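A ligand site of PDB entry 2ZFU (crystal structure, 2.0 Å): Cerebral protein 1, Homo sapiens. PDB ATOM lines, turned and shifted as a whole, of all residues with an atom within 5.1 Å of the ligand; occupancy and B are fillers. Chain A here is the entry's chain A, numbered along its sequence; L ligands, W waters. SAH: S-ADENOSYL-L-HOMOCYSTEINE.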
ATOM      1  N   SER A  22      -3.949 -32.109  28.128  1.00  0.00           N
ATOM      2  CA  SER A  22      -4.312 -30.768  28.582  1.00  0.00           C
ATOM      3  C   SER A  22      -3.087 -29.878  28.813  1.00  0.00           C
ATOM      4  O   SER A  22      -3.175 -28.666  28.663  1.00  0.00           O
ATOM      5  CB  SER A  22      -5.134 -30.851  29.865  1.00  0.00           C
ATOM      6  OG  SER A  22      -4.465 -31.620  30.830  1.00  0.00           O
ATOM      7  N   PHE A  29      -1.950 -21.924  25.073  1.00  0.00           N
ATOM      8  CA  PHE A  29      -2.682 -20.720  25.475  1.00  0.00           C
ATOM      9  C   PHE A  29      -1.884 -19.796  26.382  1.00  0.00           C
ATOM     10  O   PHE A  29      -2.079 -18.569  26.344  1.00  0.00           O
ATOM     11  CB  PHE A  29      -4.040 -21.077  26.103  1.00  0.00           C
ATOM     12  CG  PHE A  29      -5.030 -21.693  25.152  1.00  0.00           C
ATOM     13  CD1 PHE A  29      -5.126 -21.273  23.827  1.00  0.00           C
ATOM     14  CD2 PHE A  29      -5.900 -22.688  25.594  1.00  0.00           C
ATOM     15  CE1 PHE A  29      -6.032 -21.847  22.952  1.00  0.00           C
ATOM     16  CE2 PHE A  29      -6.809 -23.264  24.728  1.00  0.00           C
ATOM     17  CZ  PHE A  29      -6.873 -22.838  23.404  1.00  0.00           C
ATOM     18  N   PHE A  36      -6.246 -18.330  22.158  1.00  0.00           N
ATOM     19  CA  PHE A  36      -7.427 -18.556  22.986  1.00  0.00           C
ATOM     20  C   PHE A  36      -8.599 -17.732  22.467  1.00  0.00           C
ATOM     21  O   PHE A  36      -9.734 -18.211  22.414  1.00  0.00           O
ATOM     22  CB  PHE A  36      -7.156 -18.185  24.432  1.00  0.00           C
ATOM     23  CG  PHE A  36      -8.202 -18.677  25.404  1.00  0.00           C
ATOM     24  CD1 PHE A  36      -8.348 -20.045  25.620  1.00  0.00           C
ATOM     25  CD2 PHE A  36      -9.011 -17.792  26.091  1.00  0.00           C
ATOM     26  CE1 PHE A  36      -9.312 -20.518  26.524  1.00  0.00           C
ATOM     27  CE2 PHE A  36      -9.964 -18.258  27.000  1.00  0.00           C
ATOM     28  CZ  PHE A  36     -10.109 -19.634  27.204  1.00  0.00           C
ATOM     29  N   TYR A  39      -9.910 -19.389  19.340  1.00  0.00           N
ATOM     30  CA  TYR A  39     -10.675 -20.574  19.669  1.00  0.00           C
ATOM     31  C   TYR A  39     -12.108 -20.162  20.003  1.00  0.00           C
ATOM     32  O   TYR A  39     -13.045 -20.708  19.456  1.00  0.00           O
ATOM     33  CB  TYR A  39     -10.073 -21.365  20.856  1.00  0.00           C
ATOM     34  CG  TYR A  39     -10.996 -22.501  21.228  1.00  0.00           C
ATOM     35  CD1 TYR A  39     -11.040 -23.674  20.464  1.00  0.00           C
ATOM     36  CD2 TYR A  39     -11.924 -22.355  22.259  1.00  0.00           C
ATOM     37  CE1 TYR A  39     -11.956 -24.689  20.771  1.00  0.00           C
ATOM     38  CE2 TYR A  39     -12.816 -23.352  22.566  1.00  0.00           C
ATOM     39  CZ  TYR A  39     -12.831 -24.514  21.824  1.00  0.00           C
ATOM     40  OH  TYR A  39     -13.743 -25.482  22.154  1.00  0.00           O
ATOM     41  N   HIS A  40     -12.250 -19.172  20.872  1.00  0.00           N
ATOM     42  CA  HIS A  40     -13.572 -18.761  21.311  1.00  0.00           C
ATOM     43  C   HIS A  40     -14.380 -17.986  20.276  1.00  0.00           C
ATOM     44  O   HIS A  40     -15.600 -18.091  20.268  1.00  0.00           O
ATOM     45  CB  HIS A  40     -13.471 -18.047  22.653  1.00  0.00           C
ATOM     46  CG  HIS A  40     -13.348 -19.011  23.779  1.00  0.00           C
ATOM     47  ND1 HIS A  40     -14.412 -19.769  24.212  1.00  0.00           N
ATOM     48  CD2 HIS A  40     -12.265 -19.440  24.463  1.00  0.00           C
ATOM     49  CE1 HIS A  40     -13.993 -20.598  25.167  1.00  0.00           C
ATOM     50  NE2 HIS A  40     -12.700 -20.410  25.334  1.00  0.00           N
ATOM     51  N   PHE A  43     -15.538 -21.000  18.359  1.00  0.00           N
ATOM     52  CA  PHE A  43     -16.525 -21.732  19.152  1.00  0.00           C
ATOM     53  C   PHE A  43     -17.877 -21.014  19.175  1.00  0.00           C
ATOM     54  O   PHE A  43     -18.928 -21.628  18.965  1.00  0.00           O
ATOM     55  CB  PHE A  43     -16.000 -21.937  20.563  1.00  0.00           C
ATOM     56  CG  PHE A  43     -17.001 -22.534  21.480  1.00  0.00           C
ATOM     57  CD1 PHE A  43     -17.298 -23.898  21.409  1.00  0.00           C
ATOM     58  CD2 PHE A  43     -17.674 -21.741  22.398  1.00  0.00           C
ATOM     59  CE1 PHE A  43     -18.250 -24.448  22.245  1.00  0.00           C
ATOM     60  CE2 PHE A  43     -18.626 -22.291  23.233  1.00  0.00           C
ATOM     61  CZ  PHE A  43     -18.902 -23.649  23.169  1.00  0.00           C
ATOM     62  N   GLN A  44     -17.847 -19.701  19.404  1.00  0.00           N
ATOM     63  CA  GLN A  44     -19.069 -18.895  19.389  1.00  0.00           C
ATOM     64  C   GLN A  44     -19.758 -18.890  18.022  1.00  0.00           C
ATOM     65  O   GLN A  44     -20.991 -18.993  17.936  1.00  0.00           O
ATOM     66  CB  GLN A  44     -18.774 -17.466  19.870  1.00  0.00           C
ATOM     67  CG  GLN A  44     -18.499 -17.367  21.391  1.00  0.00           C
ATOM     68  CD  GLN A  44     -19.626 -17.948  22.233  1.00  0.00           C
ATOM     69  OE1 GLN A  44     -19.393 -18.703  23.195  1.00  0.00           O
ATOM     70  NE2 GLN A  44     -20.845 -17.645  21.843  1.00  0.00           N
ATOM     71  N   GLN A  53     -28.024 -23.967  23.152  1.00  0.00           N
ATOM     72  CA  GLN A  53     -26.727 -24.297  23.676  1.00  0.00           C
ATOM     73  C   GLN A  53     -26.790 -25.173  24.909  1.00  0.00           C
ATOM     74  O   GLN A  53     -27.691 -25.019  25.746  1.00  0.00           O
ATOM     75  CB  GLN A  53     -26.008 -23.038  24.086  1.00  0.00           C
ATOM     76  CG  GLN A  53     -25.513 -22.234  22.958  1.00  0.00           C
ATOM     77  CD  GLN A  53     -24.505 -21.231  23.442  1.00  0.00           C
ATOM     78  OE1 GLN A  53     -23.592 -21.577  24.205  1.00  0.00           O
ATOM     79  NE2 GLN A  53     -24.669 -19.970  23.038  1.00  0.00           N
ATOM     80  N   VAL A  55     -24.883 -24.985  27.596  1.00  0.00           N
ATOM     81  CA  VAL A  55     -24.806 -24.180  28.846  1.00  0.00           C
ATOM     82  C   VAL A  55     -26.164 -23.727  29.339  1.00  0.00           C
ATOM     83  O   VAL A  55     -26.364 -23.614  30.536  1.00  0.00           O
ATOM     84  CB  VAL A  55     -24.029 -22.820  28.828  1.00  0.00           C
ATOM     85  CG1 VAL A  55     -22.898 -22.822  29.831  1.00  0.00           C
ATOM     86  CG2 VAL A  55     -23.688 -22.325  27.486  1.00  0.00           C
ATOM     87  N   ASP A  73     -17.632 -25.094  37.393  1.00  0.00           N
ATOM     88  CA  ASP A  73     -17.762 -25.071  35.932  1.00  0.00           C
ATOM     89  C   ASP A  73     -16.373 -25.368  35.390  1.00  0.00           C
ATOM     90  O   ASP A  73     -15.485 -24.499  35.392  1.00  0.00           O
ATOM     91  CB  ASP A  73     -18.312 -23.705  35.475  1.00  0.00           C
ATOM     92  CG  ASP A  73     -18.710 -23.677  34.003  1.00  0.00           C
ATOM     93  OD1 ASP A  73     -18.721 -24.733  33.330  1.00  0.00           O
ATOM     94  OD2 ASP A  73     -19.029 -22.562  33.519  1.00  0.00           O
ATOM     95  N   GLY A  75     -13.947 -25.886  32.636  1.00  0.00           N
ATOM     96  CA  GLY A  75     -13.819 -25.388  31.266  1.00  0.00           C
ATOM     97  C   GLY A  75     -14.910 -24.398  30.981  1.00  0.00           C
ATOM     98  O   GLY A  75     -15.700 -24.587  30.061  1.00  0.00           O
ATOM     99  N   CYS A  76     -14.926 -23.312  31.750  1.00  0.00           N
ATOM    100  CA  CYS A  76     -16.053 -22.396  31.821  1.00  0.00           C
ATOM    101  C   CYS A  76     -16.192 -21.415  30.642  1.00  0.00           C
ATOM    102  O   CYS A  76     -17.225 -20.756  30.507  1.00  0.00           O
ATOM    103  CB  CYS A  76     -15.936 -21.562  33.101  1.00  0.00           C
ATOM    104  SG  CYS A  76     -14.375 -20.649  33.208  1.00  0.00           S
ATOM    105  N   GLY A  77     -15.128 -21.267  29.848  1.00  0.00           N
ATOM    106  CA  GLY A  77     -15.091 -20.275  28.774  1.00  0.00           C
ATOM    107  C   GLY A  77     -15.469 -18.920  29.302  1.00  0.00           C
ATOM    108  O   GLY A  77     -14.902 -18.450  30.291  1.00  0.00           O
ATOM    109  N   ASP A  78     -16.472 -18.286  28.711  1.00  0.00           N
ATOM    110  CA  ASP A  78     -16.832 -16.924  29.129  1.00  0.00           C
ATOM    111  C   ASP A  78     -17.891 -16.850  30.254  1.00  0.00           C
ATOM    112  O   ASP A  78     -18.503 -15.806  30.460  1.00  0.00           O
ATOM    113  CB  ASP A  78     -17.212 -16.093  27.919  1.00  0.00           C
ATOM    114  CG  ASP A  78     -18.547 -16.439  27.362  1.00  0.00           C
ATOM    115  OD1 ASP A  78     -19.027 -15.616  26.570  1.00  0.00           O
ATOM    116  OD2 ASP A  78     -19.127 -17.490  27.723  1.00  0.00           O
ATOM    117  N   PHE A  92     -13.446 -22.483  36.092  1.00  0.00           N
ATOM    118  CA  PHE A  92     -12.098 -22.949  35.765  1.00  0.00           C
ATOM    119  C   PHE A  92     -11.872 -23.033  34.262  1.00  0.00           C
ATOM    120  O   PHE A  92     -12.670 -23.612  33.544  1.00  0.00           O
ATOM    121  CB  PHE A  92     -11.890 -24.316  36.381  1.00  0.00           C
ATOM    122  CG  PHE A  92     -12.050 -24.333  37.878  1.00  0.00           C
ATOM    123  CD1 PHE A  92     -13.048 -25.084  38.482  1.00  0.00           C
ATOM    124  CD2 PHE A  92     -11.203 -23.563  38.677  1.00  0.00           C
ATOM    125  CE1 PHE A  92     -13.190 -25.085  39.871  1.00  0.00           C
ATOM    126  CE2 PHE A  92     -11.326 -23.567  40.071  1.00  0.00           C
ATOM    127  CZ  PHE A  92     -12.323 -24.326  40.662  1.00  0.00           C
ATOM    128  N   ASP A  93     -10.769 -22.445  33.788  1.00  0.00           N
ATOM    129  CA  ASP A  93     -10.382 -22.599  32.388  1.00  0.00           C
ATOM    130  C   ASP A  93      -8.895 -22.345  32.231  1.00  0.00           C
ATOM    131  O   ASP A  93      -8.238 -21.823  33.140  1.00  0.00           O
ATOM    132  CB  ASP A  93     -11.237 -21.652  31.510  1.00  0.00           C
ATOM    133  CG  ASP A  93     -11.363 -22.137  30.066  1.00  0.00           C
ATOM    134  OD1 ASP A  93     -12.510 -22.234  29.579  1.00  0.00           O
ATOM    135  OD2 ASP A  93     -10.329 -22.392  29.423  1.00  0.00           O
ATOM    136  N   LEU A  94      -8.357 -22.729  31.064  1.00  0.00           N
ATOM    137  CA  LEU A  94      -6.926 -22.600  30.776  1.00  0.00           C
ATOM    138  C   LEU A  94      -6.471 -21.145  30.561  1.00  0.00           C
ATOM    139  O   LEU A  94      -5.272 -20.846  30.557  1.00  0.00           O
ATOM    140  CB  LEU A  94      -6.557 -23.420  29.531  1.00  0.00           C
ATOM    141  CG  LEU A  94      -6.699 -24.939  29.606  1.00  0.00           C
ATOM    142  CD1 LEU A  94      -6.640 -25.542  28.208  1.00  0.00           C
ATOM    143  CD2 LEU A  94      -5.638 -25.559  30.536  1.00  0.00           C
ATOM    144  N   CYS A 104      -6.368 -22.305  35.358  1.00  0.00           N
ATOM    145  CA  CYS A 104      -5.712 -23.538  35.738  1.00  0.00           C
ATOM    146  C   CYS A 104      -6.044 -24.616  34.723  1.00  0.00           C
ATOM    147  O   CYS A 104      -6.933 -24.452  33.892  1.00  0.00           O
ATOM    148  CB  CYS A 104      -6.182 -23.998  37.126  1.00  0.00           C
ATOM    149  SG  CYS A 104      -7.962 -24.343  37.296  1.00  0.00           S
ATOM    150  N   ASP A 105      -5.320 -25.719  34.791  1.00  0.00           N
ATOM    151  CA  ASP A 105      -5.756 -26.976  34.205  1.00  0.00           C
ATOM    152  C   ASP A 105      -6.791 -27.607  35.147  1.00  0.00           C
ATOM    153  O   ASP A 105      -6.526 -27.802  36.338  1.00  0.00           O
ATOM    154  CB  ASP A 105      -4.580 -27.905  34.006  1.00  0.00           C
ATOM    155  CG  ASP A 105      -4.934 -29.156  33.210  1.00  0.00           C
ATOM    156  OD1 ASP A 105      -6.126 -29.536  33.122  1.00  0.00           O
ATOM    157  OD2 ASP A 105      -3.993 -29.756  32.682  1.00  0.00           O
ATOM    158  N   MET A 106      -7.954 -27.924  34.592  1.00  0.00           N
ATOM    159  CA  MET A 106      -9.080 -28.415  35.371  1.00  0.00           C
ATOM    160  C   MET A 106      -8.854 -29.853  35.857  1.00  0.00           C
ATOM    161  O   MET A 106      -9.593 -30.343  36.682  1.00  0.00           O
ATOM    162  CB  MET A 106     -10.373 -28.258  34.561  1.00  0.00           C
ATOM    163  CG  MET A 106     -10.550 -29.280  33.423  1.00  0.00           C
ATOM    164  SD  MET A 106     -11.811 -28.858  32.207  1.00  0.00           S
ATOM    165  CE  MET A 106     -11.703 -30.369  31.234  1.00  0.00           C
ATOM    166  N   ALA A 107      -7.801 -30.494  35.351  1.00  0.00           N
ATOM    167  CA  ALA A 107      -7.285 -31.731  35.925  1.00  0.00           C
ATOM    168  C   ALA A 107      -6.846 -31.527  37.368  1.00  0.00           C
ATOM    169  O   ALA A 107      -6.800 -32.473  38.125  1.00  0.00           O
ATOM    170  CB  ALA A 107      -6.112 -32.213  35.128  1.00  0.00           C
ATOM    171  N   CYS A 122     -19.269 -28.736  30.249  1.00  0.00           N
ATOM    172  CA  CYS A 122     -20.100 -28.361  29.122  1.00  0.00           C
ATOM    173  C   CYS A 122     -19.234 -28.107  27.882  1.00  0.00           C
ATOM    174  O   CYS A 122     -18.685 -27.013  27.682  1.00  0.00           O
ATOM    175  CB  CYS A 122     -20.935 -27.135  29.490  1.00  0.00           C
ATOM    176  SG  CYS A 122     -22.094 -26.593  28.246  1.00  0.00           S
ATOM    177  N   LEU A 123     -19.094 -29.152  27.062  1.00  0.00           N
ATOM    178  CA  LEU A 123     -18.284 -29.115  25.839  1.00  0.00           C
ATOM    179  C   LEU A 123     -16.779 -28.898  26.105  1.00  0.00           C
ATOM    180  O   LEU A 123     -16.058 -28.376  25.250  1.00  0.00           O
ATOM    181  CB  LEU A 123     -18.789 -28.034  24.878  1.00  0.00           C
ATOM    182  CG  LEU A 123     -20.265 -28.024  24.494  1.00  0.00           C
ATOM    183  CD1 LEU A 123     -20.519 -26.940  23.488  1.00  0.00           C
ATOM    184  CD2 LEU A 123     -20.733 -29.401  23.945  1.00  0.00           C
ATOM    185  N   SER A 124     -16.315 -29.341  27.271  1.00  0.00           N
ATOM    186  CA  SER A 124     -14.984 -29.004  27.751  1.00  0.00           C
ATOM    187  C   SER A 124     -14.004 -30.176  27.875  1.00  0.00           C
ATOM    188  O   SER A 124     -12.825 -29.943  28.159  1.00  0.00           O
ATOM    189  CB  SER A 124     -15.073 -28.297  29.091  1.00  0.00           C
ATOM    190  OG  SER A 124     -15.618 -29.124  30.103  1.00  0.00           O
ATOM    191  N   MET A 126     -11.790 -31.863  26.390  1.00  0.00           N
ATOM    192  CA  MET A 126     -11.096 -31.751  25.099  1.00  0.00           C
ATOM    193  C   MET A 126      -9.846 -32.603  25.003  1.00  0.00           C
ATOM    194  O   MET A 126      -9.688 -33.359  24.034  1.00  0.00           O
ATOM    195  CB  MET A 126     -10.750 -30.287  24.824  1.00  0.00           C
ATOM    196  CG  MET A 126     -11.996 -29.407  24.704  1.00  0.00           C
ATOM    197  SD  MET A 126     -11.593 -27.725  24.145  1.00  0.00           S
ATOM    198  CE  MET A 126     -11.271 -28.046  22.398  1.00  0.00           C
ATOM    199  N   GLY A 127      -8.968 -32.518  25.998  1.00  0.00           N
ATOM    200  CA  GLY A 127      -7.682 -33.213  25.919  1.00  0.00           C
ATOM    201  C   GLY A 127      -7.769 -34.725  25.946  1.00  0.00           C
ATOM    202  O   GLY A 127      -8.790 -35.275  26.325  1.00  0.00           O
ATOM    203  N   PHE A 133      -9.667 -35.385  34.200  1.00  0.00           N
ATOM    204  CA  PHE A 133     -10.694 -34.374  34.451  1.00  0.00           C
ATOM    205  C   PHE A 133     -11.787 -34.958  35.324  1.00  0.00           C
ATOM    206  O   PHE A 133     -12.211 -34.336  36.292  1.00  0.00           O
ATOM    207  CB  PHE A 133     -11.315 -33.848  33.132  1.00  0.00           C
ATOM    208  CG  PHE A 133     -10.298 -33.437  32.089  1.00  0.00           C
ATOM    209  CD1 PHE A 133     -10.514 -33.718  30.744  1.00  0.00           C
ATOM    210  CD2 PHE A 133      -9.112 -32.799  32.451  1.00  0.00           C
ATOM    211  CE1 PHE A 133      -9.596 -33.355  29.769  1.00  0.00           C
ATOM    212  CE2 PHE A 133      -8.183 -32.428  31.481  1.00  0.00           C
ATOM    213  CZ  PHE A 133      -8.420 -32.707  30.141  1.00  0.00           C
HETATM  214  N   SAH L   1     -18.393 -24.419  28.901  1.00  0.00           N
HETATM  215  CA  SAH L   1     -18.278 -23.228  28.057  1.00  0.00           C
HETATM  216  CB  SAH L   1     -17.042 -23.301  27.152  1.00  0.00           C
HETATM  217  CG  SAH L   1     -16.973 -24.500  26.200  1.00  0.00           C
HETATM  218  SD  SAH L   1     -15.621 -24.408  24.984  1.00  0.00           S
HETATM  219  C   SAH L   1     -19.514 -23.001  27.195  1.00  0.00           C
HETATM  220  O   SAH L   1     -20.320 -23.928  27.021  1.00  0.00           O
HETATM  221  OXT SAH L   1     -19.726 -21.902  26.642  1.00  0.00           O
HETATM  222  C5' SAH L   1     -14.468 -25.485  25.863  1.00  0.00           C
HETATM  223  C4' SAH L   1     -13.685 -24.800  26.996  1.00  0.00           C
HETATM  224  O4' SAH L   1     -13.071 -25.805  27.782  1.00  0.00           O
HETATM  225  C3' SAH L   1     -12.573 -23.863  26.502  1.00  0.00           C
HETATM  226  O3' SAH L   1     -12.696 -22.588  27.126  1.00  0.00           O
HETATM  227  C2' SAH L   1     -11.312 -24.575  26.913  1.00  0.00           C
HETATM  228  O2' SAH L   1     -10.183 -23.746  27.144  1.00  0.00           O
HETATM  229  C1' SAH L   1     -11.804 -25.327  28.160  1.00  0.00           C
HETATM  230  N9  SAH L   1     -10.879 -26.380  28.522  1.00  0.00           N
HETATM  231  C8  SAH L   1     -10.518 -27.440  27.729  1.00  0.00           C
HETATM  232  N7  SAH L   1      -9.630 -28.162  28.426  1.00  0.00           N
HETATM  233  C5  SAH L   1      -9.414 -27.597  29.647  1.00  0.00           C
HETATM  234  C6  SAH L   1      -8.613 -27.957  30.738  1.00  0.00           C
HETATM  235  N6  SAH L   1      -7.848 -29.035  30.695  1.00  0.00           N
HETATM  236  N1  SAH L   1      -8.614 -27.161  31.868  1.00  0.00           N
HETATM  237  C2  SAH L   1      -9.406 -26.042  31.923  1.00  0.00           C
HETATM  238  N3  SAH L   1     -10.219 -25.682  30.840  1.00  0.00           N
HETATM  239  C4  SAH L   1     -10.206 -26.461  29.717  1.00  0.00           C
HETATM  240  O   HOH W   1     -19.700 -19.932  28.691  1.00  0.00           O
HETATM  241  O   HOH W   2     -21.211 -20.373  25.191  1.00  0.00           O
HETATM  242  O   HOH W   3     -20.255 -23.949  31.003  1.00  0.00           O
HETATM  243  O   HOH W   4     -17.756 -19.866  26.506  1.00  0.00           O
HETATM  244  O   HOH W   5     -17.880 -26.413  31.383  1.00  0.00           O
HETATM  245  O   HOH W   6     -22.763 -24.110  25.581  1.00  0.00           O
HETATM  246  O   HOH W   7      -7.919 -30.114  27.748  1.00  0.00           O
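O of Gly 75 sits at hydrogen-bond distance from N of the ligand, 2.9 Å away.
N6 of the ligand sits at hydrogen-bond distance from OD1 of Asp 105, at 3.0 Å.
A ring nitrogen (NE2) of His 40 sits at hydrogen-bond distance from an oxygen (O3') of the ligand.
OD1 of Asp 93 is in hydrogen-bond range of O3' of the ligand (2.5 Å).
The backbone NH (N) of Met 106 is in hydrogen-bond range of a nitrogen (N1) of the ligand (2.9 Å).
The backbone carbonyl oxygen of Cys 122 lies within hydrogen-bond range of a nitrogen (N) of the ligand.
The side-chain hydroxyl (OH) of Tyr 39 lies close to a sulfur (SD) of the ligand (3.6 Å).
N3 of the ligand is in hydrogen-bond range of N of Leu 94.
SG of Cys 122 is in hydrogen-bond range of O of the ligand, at 3.4 Å.
The side-chain hydroxyl (OG) of Ser 22 lies within hydrogen-bond range of the side-chain carboxylate (OD2) of Asp 105 (2.7 Å).
O of Phe 92 lies within hydrogen-bond range of N of Cys 76 (2.9 Å).
The side-chain carboxylate (OD1) of Asp 105 sits at hydrogen-bond distance from the backbone NH (N) of Ala 107, 2.9 Å away.
OD1 of Asp 93 lies within hydrogen-bond range of N of Gly 77 (2.8 Å).
The backbone NH (N) of Cys 76 is in hydrogen-bond range of the side-chain carboxylate (OD1) of Asp 93 (3.4 Å).
SD of Met 126 sits close to OH of Tyr 39, 3.7 Å away.
The backbone NH of Cys 104 lies within hydrogen-bond range of the backbone carbonyl oxygen of Asp 93.
The backbone NH (N) of Gly 75 lies within hydrogen-bond range of the backbone carbonyl oxygen (O) of Phe 92.
Merely in contact with the ligand: Ser 22, Phe 36, Phe 43, Val 55, Cys 76, Gly 77, Cys 104, Leu 123, Ser 124, Met 126 and Phe 133.
Hydrophobic or aromatic side chains within 4 Å of the ligand: Phe 36, Tyr 39, His 40, Phe 43, Val 55, Leu 94, Met 106, Met 126 and Phe 133.
19 residues have an atom within 4 Å of the ligand: Ser 22, Phe 36, Tyr 39, His 40, Phe 43, Val 55, Gly 75, Cys 76, Gly 77, Asp 93, Leu 94, Cys 104, Asp 105, Met 106, Cys 122, Leu 123, Ser 124, Met 126 and Phe 133.
Along chain A the residues within 4 Å of the ligand span positions 22 to 133.
The nearest printed residue that does not touch the ligand is Phe 29 (4.2 Å).
Water W2 lies within hydrogen-bond range of OXT of the ligand (2.6 Å), OE1 of Gln 53 (2.8 Å) and OE1 of Gln 44 (3.2 Å).
Water W7 bridges a nitrogen (N7) of the ligand (2.7 Å) and the backbone NH (N) of Gly 127 (3.2 Å).
Water W4 lies within hydrogen-bond range of OXT of the ligand (2.8 Å) and OD2 of Asp 78 (3.0 Å).
Water W1 lies within hydrogen-bond range of the side-chain carboxylate (OD2) of Asp 78 (2.7 Å), an oxygen (OXT) of the ligand (2.8 Å) and the backbone carbonyl oxygen (O) of Cys 76 (3.2 Å).
Water W3 bridges N of the ligand and OD1 of Asp 73.
Water W5 lies within hydrogen-bond range of OD1 of Asp 73 (2.7 Å), N of Cys 122 (2.9 Å), O of Gly 75 (3.1 Å) and N of the ligand (3.2 Å).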
